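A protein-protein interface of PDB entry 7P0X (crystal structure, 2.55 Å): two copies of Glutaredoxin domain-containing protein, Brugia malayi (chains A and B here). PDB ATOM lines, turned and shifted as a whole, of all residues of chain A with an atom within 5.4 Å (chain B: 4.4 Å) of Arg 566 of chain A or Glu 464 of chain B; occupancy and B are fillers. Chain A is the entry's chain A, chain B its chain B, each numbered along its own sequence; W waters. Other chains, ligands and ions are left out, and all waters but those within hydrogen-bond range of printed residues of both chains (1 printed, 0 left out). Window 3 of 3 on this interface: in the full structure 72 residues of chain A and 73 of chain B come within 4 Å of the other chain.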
ATOM      1  N   LYS A 561     -11.459 -15.300 -30.469  1.00  0.00           N
ATOM      2  CA  LYS A 561     -11.267 -16.292 -31.569  1.00  0.00           C
ATOM      3  C   LYS A 561     -10.517 -17.540 -31.043  1.00  0.00           C
ATOM      4  O   LYS A 561     -10.946 -18.703 -31.307  1.00  0.00           O
ATOM      5  CB  LYS A 561     -10.541 -15.572 -32.700  1.00  0.00           C
ATOM      6  CG  LYS A 561     -10.169 -16.424 -33.898  1.00  0.00           C
ATOM      7  CD  LYS A 561     -11.338 -17.074 -34.567  1.00  0.00           C
ATOM      8  CE  LYS A 561     -10.975 -17.588 -35.949  1.00  0.00           C
ATOM      9  NZ  LYS A 561      -9.748 -18.414 -35.910  1.00  0.00           N
ATOM     10  N   ALA A 562      -9.450 -17.327 -30.286  1.00  0.00           N
ATOM     11  CA  ALA A 562      -8.595 -18.387 -29.696  1.00  0.00           C
ATOM     12  C   ALA A 562      -9.423 -19.390 -28.881  1.00  0.00           C
ATOM     13  O   ALA A 562      -9.030 -20.553 -28.837  1.00  0.00           O
ATOM     14  CB  ALA A 562      -7.511 -17.776 -28.844  1.00  0.00           C
ATOM     15  N   ASP A 563     -10.518 -18.952 -28.271  1.00  0.00           N
ATOM     16  CA  ASP A 563     -11.421 -19.826 -27.483  1.00  0.00           C
ATOM     17  C   ASP A 563     -12.221 -20.700 -28.455  1.00  0.00           C
ATOM     18  O   ASP A 563     -12.479 -21.863 -28.139  1.00  0.00           O
ATOM     19  CB  ASP A 563     -12.313 -18.973 -26.574  1.00  0.00           C
ATOM     20  CG  ASP A 563     -11.512 -18.249 -25.507  1.00  0.00           C
ATOM     21  OD1 ASP A 563     -10.717 -18.919 -24.848  1.00  0.00           O
ATOM     22  OD2 ASP A 563     -11.658 -17.014 -25.361  1.00  0.00           O
ATOM     23  N   PHE A 564     -12.642 -20.139 -29.588  1.00  0.00           N
ATOM     24  CA  PHE A 564     -13.354 -20.897 -30.635  1.00  0.00           C
ATOM     25  C   PHE A 564     -12.355 -21.893 -31.214  1.00  0.00           C
ATOM     26  O   PHE A 564     -12.746 -23.032 -31.392  1.00  0.00           O
ATOM     27  CB  PHE A 564     -13.983 -19.962 -31.657  1.00  0.00           C
ATOM     28  CG  PHE A 564     -15.362 -19.478 -31.301  1.00  0.00           C
ATOM     29  CD1 PHE A 564     -15.625 -18.945 -30.064  1.00  0.00           C
ATOM     30  CD2 PHE A 564     -16.385 -19.533 -32.216  1.00  0.00           C
ATOM     31  CE1 PHE A 564     -16.887 -18.483 -29.738  1.00  0.00           C
ATOM     32  CE2 PHE A 564     -17.651 -19.065 -31.890  1.00  0.00           C
ATOM     33  CZ  PHE A 564     -17.900 -18.544 -30.650  1.00  0.00           C
ATOM     34  N   ASP A 565     -11.081 -21.512 -31.358  1.00  0.00           N
ATOM     35  CA  ASP A 565     -10.074 -22.391 -32.009  1.00  0.00           C
ATOM     36  C   ASP A 565      -9.664 -23.548 -31.087  1.00  0.00           C
ATOM     37  O   ASP A 565      -9.196 -24.560 -31.601  1.00  0.00           O
ATOM     38  CB  ASP A 565      -8.868 -21.582 -32.484  1.00  0.00           C
ATOM     39  CG  ASP A 565      -9.200 -20.632 -33.633  1.00  0.00           C
ATOM     40  OD1 ASP A 565     -10.244 -20.834 -34.299  1.00  0.00           O
ATOM     41  OD2 ASP A 565      -8.428 -19.679 -33.860  1.00  0.00           O
ATOM     42  N   ARG A 566      -9.770 -23.440 -29.764  1.00  0.00           N
ATOM     43  CA  ARG A 566      -9.268 -24.507 -28.863  1.00  0.00           C
ATOM     44  C   ARG A 566     -10.457 -25.406 -28.451  1.00  0.00           C
ATOM     45  O   ARG A 566     -10.264 -26.417 -27.768  1.00  0.00           O
ATOM     46  CB  ARG A 566      -8.491 -23.879 -27.707  1.00  0.00           C
ATOM     47  CG  ARG A 566      -9.333 -23.211 -26.634  1.00  0.00           C
ATOM     48  CD  ARG A 566      -8.504 -22.245 -25.794  1.00  0.00           C
ATOM     49  NE  ARG A 566      -9.306 -21.428 -24.890  1.00  0.00           N
ATOM     50  CZ  ARG A 566      -9.580 -21.717 -23.613  1.00  0.00           C
ATOM     51  NH1 ARG A 566      -9.159 -22.835 -23.064  1.00  0.00           N
ATOM     52  NH2 ARG A 566     -10.309 -20.884 -22.889  1.00  0.00           N
ATOM     53  N   LEU A 567     -11.664 -25.019 -28.830  1.00  0.00           N
ATOM     54  CA  LEU A 567     -12.861 -25.853 -28.653  1.00  0.00           C
ATOM     55  C   LEU A 567     -12.764 -26.970 -29.693  1.00  0.00           C
ATOM     56  O   LEU A 567     -12.571 -26.633 -30.870  1.00  0.00           O
ATOM     57  CB  LEU A 567     -14.096 -24.979 -28.865  1.00  0.00           C
ATOM     58  CG  LEU A 567     -15.431 -25.710 -28.846  1.00  0.00           C
ATOM     59  CD1 LEU A 567     -15.705 -26.305 -27.490  1.00  0.00           C
ATOM     60  CD2 LEU A 567     -16.538 -24.778 -29.256  1.00  0.00           C
ATOM     61  N   ILE A 568     -12.870 -28.225 -29.266  1.00  0.00           N
ATOM     62  CA  ILE A 568     -12.801 -29.389 -30.171  1.00  0.00           C
ATOM     63  C   ILE A 568     -14.176 -29.586 -30.792  1.00  0.00           C
ATOM     64  O   ILE A 568     -15.171 -29.537 -30.079  1.00  0.00           O
ATOM     65  CB  ILE A 568     -12.317 -30.649 -29.460  1.00  0.00           C
ATOM     66  CG1 ILE A 568     -11.014 -30.409 -28.694  1.00  0.00           C
ATOM     67  CG2 ILE A 568     -12.203 -31.749 -30.483  1.00  0.00           C
ATOM     68  CD1 ILE A 568      -9.881 -29.984 -29.558  1.00  0.00           C
ATOM     69  N   GLN B 446      -6.969 -31.613 -34.638  1.00  0.00           N
ATOM     70  CA  GLN B 446      -6.413 -30.514 -33.808  1.00  0.00           C
ATOM     71  C   GLN B 446      -4.982 -30.878 -33.371  1.00  0.00           C
ATOM     72  O   GLN B 446      -4.084 -29.990 -33.448  1.00  0.00           O
ATOM     73  CB  GLN B 446      -7.341 -30.278 -32.599  1.00  0.00           C
ATOM     74  CG  GLN B 446      -6.877 -29.204 -31.618  1.00  0.00           C
ATOM     75  CD  GLN B 446      -7.042 -27.817 -32.169  1.00  0.00           C
ATOM     76  OE1 GLN B 446      -7.005 -27.607 -33.361  1.00  0.00           O
ATOM     77  NE2 GLN B 446      -7.304 -26.867 -31.305  1.00  0.00           N
ATOM     78  N   LEU B 462      -0.933 -26.045 -26.777  1.00  0.00           N
ATOM     79  CA  LEU B 462      -1.247 -27.462 -26.461  1.00  0.00           C
ATOM     80  C   LEU B 462      -2.657 -27.767 -26.944  1.00  0.00           C
ATOM     81  O   LEU B 462      -3.532 -26.908 -26.803  1.00  0.00           O
ATOM     82  CB  LEU B 462      -1.152 -27.696 -24.958  1.00  0.00           C
ATOM     83  CG  LEU B 462       0.061 -27.070 -24.287  1.00  0.00           C
ATOM     84  CD1 LEU B 462       0.035 -27.373 -22.785  1.00  0.00           C
ATOM     85  CD2 LEU B 462       1.341 -27.571 -24.964  1.00  0.00           C
ATOM     86  N   THR B 463      -2.870 -28.957 -27.470  1.00  0.00           N
ATOM     87  CA  THR B 463      -4.220 -29.489 -27.714  1.00  0.00           C
ATOM     88  C   THR B 463      -4.889 -29.693 -26.360  1.00  0.00           C
ATOM     89  O   THR B 463      -4.239 -30.205 -25.457  1.00  0.00           O
ATOM     90  CB  THR B 463      -4.139 -30.770 -28.531  1.00  0.00           C
ATOM     91  OG1 THR B 463      -3.641 -30.341 -29.794  1.00  0.00           O
ATOM     92  CG2 THR B 463      -5.480 -31.476 -28.623  1.00  0.00           C
ATOM     93  N   GLU B 464      -6.143 -29.296 -26.228  1.00  0.00           N
ATOM     94  CA  GLU B 464      -6.942 -29.500 -24.998  1.00  0.00           C
ATOM     95  C   GLU B 464      -7.740 -30.797 -25.167  1.00  0.00           C
ATOM     96  O   GLU B 464      -8.636 -30.848 -26.022  1.00  0.00           O
ATOM     97  CB  GLU B 464      -7.721 -28.215 -24.739  1.00  0.00           C
ATOM     98  CG  GLU B 464      -6.776 -27.036 -24.499  1.00  0.00           C
ATOM     99  CD  GLU B 464      -7.418 -25.682 -24.187  1.00  0.00           C
ATOM    100  OE1 GLU B 464      -8.656 -25.570 -24.299  1.00  0.00           O
ATOM    101  OE2 GLU B 464      -6.670 -24.726 -23.865  1.00  0.00           O
ATOM    102  N   TYR B 465      -7.333 -31.821 -24.417  1.00  0.00           N
ATOM    103  CA  TYR B 465      -7.839 -33.218 -24.452  1.00  0.00           C
ATOM    104  C   TYR B 465      -8.913 -33.425 -23.377  1.00  0.00           C
ATOM    105  O   TYR B 465      -9.523 -34.480 -23.365  1.00  0.00           O
ATOM    106  CB  TYR B 465      -6.664 -34.187 -24.285  1.00  0.00           C
ATOM    107  CG  TYR B 465      -5.731 -34.287 -25.471  1.00  0.00           C
ATOM    108  CD1 TYR B 465      -6.088 -35.011 -26.607  1.00  0.00           C
ATOM    109  CD2 TYR B 465      -4.452 -33.735 -25.445  1.00  0.00           C
ATOM    110  CE1 TYR B 465      -5.223 -35.147 -27.686  1.00  0.00           C
ATOM    111  CE2 TYR B 465      -3.589 -33.844 -26.526  1.00  0.00           C
ATOM    112  CZ  TYR B 465      -3.969 -34.574 -27.645  1.00  0.00           C
ATOM    113  OH  TYR B 465      -3.161 -34.678 -28.744  1.00  0.00           O
ATOM    114  N   ASP B 466      -9.191 -32.423 -22.534  1.00  0.00           N
ATOM    115  CA  ASP B 466     -10.247 -32.517 -21.494  1.00  0.00           C
ATOM    116  C   ASP B 466     -11.544 -31.854 -22.007  1.00  0.00           C
ATOM    117  O   ASP B 466     -11.485 -31.006 -22.914  1.00  0.00           O
ATOM    118  CB  ASP B 466      -9.736 -31.979 -20.153  1.00  0.00           C
ATOM    119  CG  ASP B 466      -9.383 -30.497 -20.153  1.00  0.00           C
ATOM    120  OD1 ASP B 466      -8.875 -30.024 -21.215  1.00  0.00           O
ATOM    121  OD2 ASP B 466      -9.595 -29.825 -19.082  1.00  0.00           O
ATOM    122  N   ILE B 468     -14.008 -32.626 -23.885  1.00  0.00           N
ATOM    123  CA  ILE B 468     -14.267 -32.748 -25.335  1.00  0.00           C
ATOM    124  C   ILE B 468     -15.724 -33.156 -25.509  1.00  0.00           C
ATOM    125  O   ILE B 468     -16.156 -34.171 -24.972  1.00  0.00           O
ATOM    126  CB  ILE B 468     -13.287 -33.748 -25.974  1.00  0.00           C
ATOM    127  CG1 ILE B 468     -11.878 -33.157 -26.006  1.00  0.00           C
ATOM    128  CG2 ILE B 468     -13.761 -34.138 -27.365  1.00  0.00           C
ATOM    129  CD1 ILE B 468     -10.804 -34.154 -26.376  1.00  0.00           C
ATOM    130  N   LYS B 556     -14.857 -24.353 -20.972  1.00  0.00           N
ATOM    131  CA  LYS B 556     -13.540 -23.678 -21.136  1.00  0.00           C
ATOM    132  C   LYS B 556     -13.462 -22.414 -20.265  1.00  0.00           C
ATOM    133  O   LYS B 556     -12.355 -21.864 -20.117  1.00  0.00           O
ATOM    134  CB  LYS B 556     -13.326 -23.236 -22.588  1.00  0.00           C
ATOM    135  CG  LYS B 556     -13.359 -24.331 -23.651  1.00  0.00           C
ATOM    136  CD  LYS B 556     -12.335 -25.420 -23.457  1.00  0.00           C
ATOM    137  CE  LYS B 556     -11.841 -25.927 -24.799  1.00  0.00           C
ATOM    138  NZ  LYS B 556     -11.028 -27.159 -24.717  1.00  0.00           N
HETATM  139  O   HOH W   1     -13.304 -28.820 -26.436  1.00  0.00           O
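No position is printed for both chains.
Of the 8 pairs that touch across the chains among the printed residues, none has its exchanged pair printed and touching as well.
Gln 446 of chain B touches Arg 566 of chain A.
Leu 567 of chain A touches Lys 556 of chain B (CA to CE, 3.99 Å).
CD1 of Ile 568 of chain A touches CG of Gln 446 of chain B, at 3.7 Å.
O of Glu 464 of chain B touches CG1 of Ile 568 of chain A, at 3.6 Å.
CG1 of Ile 468 of chain B touches CG1 of Ile 568 of chain A, 3.9 Å away.
Water W1 bridges the backbone NH (N) of Ile 568 of chain A and the side-chain amino group (NZ) of Lys 556 of chain B.
The side-chain carboxylate of Glu 464 of chain B lies within salt-bridge range of the side-chain amino group of Lys 556 of chain B, at 2.9 Å.
The guanidinium group of Arg 566 of chain A lies within salt-bridge range of the side-chain carboxylate of Asp 563 of chain A, at 2.8 Å.
The side-chain carboxylate of Asp 565 of chain A lies within salt-bridge range of the side-chain amino group of Lys 561 of chain A, 2.7 Å away.
Glu 464 of chain B touches two residues of chain A.
Of the printed residues of chain B, Leu 567 of chain A touches Lys 556 (3.99 Å).
Of the printed residues of chain B, Ile 568 of chain A touches Gln 446 (3.7 Å), Glu 464 (3.6 Å) and Ile 468 (3.9 Å).
Lys 561 of chain A touches none of the printed residues of chain B.
The nearest printed residue of chain B that does not touch Arg 566 of chain A is Leu 462 of chain B (5.9 Å).
The nearest printed residue of chain A that does not touch Lys 556 of chain B is Ile 568 of chain A (5.0 Å).
O of Arg 566 of chain A lies within hydrogen-bond range of NZ of Lys 556 of chain B.
OE1 of Glu 464 of chain B lies within salt-bridge range of NH1 of Arg 566 of chain A (3.0 Å).
NE2 of Gln 446 of chain B lies within hydrogen-bond range of O of Asp 565 of chain A, 3.0 Å away.
Of the 8 printed residues of chain B, 4 touch a printed residue of chain A.
Printed residues of chain B that touch a printed residue of chain A: Gln 446, Glu 464, Ile 468 and Lys 556.
Hydrophobic or aromatic side chains of chain B that line the printed part of chain A: Ile 468.
Of the 8 printed residues of chain A, 4 touch a printed residue of chain B.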
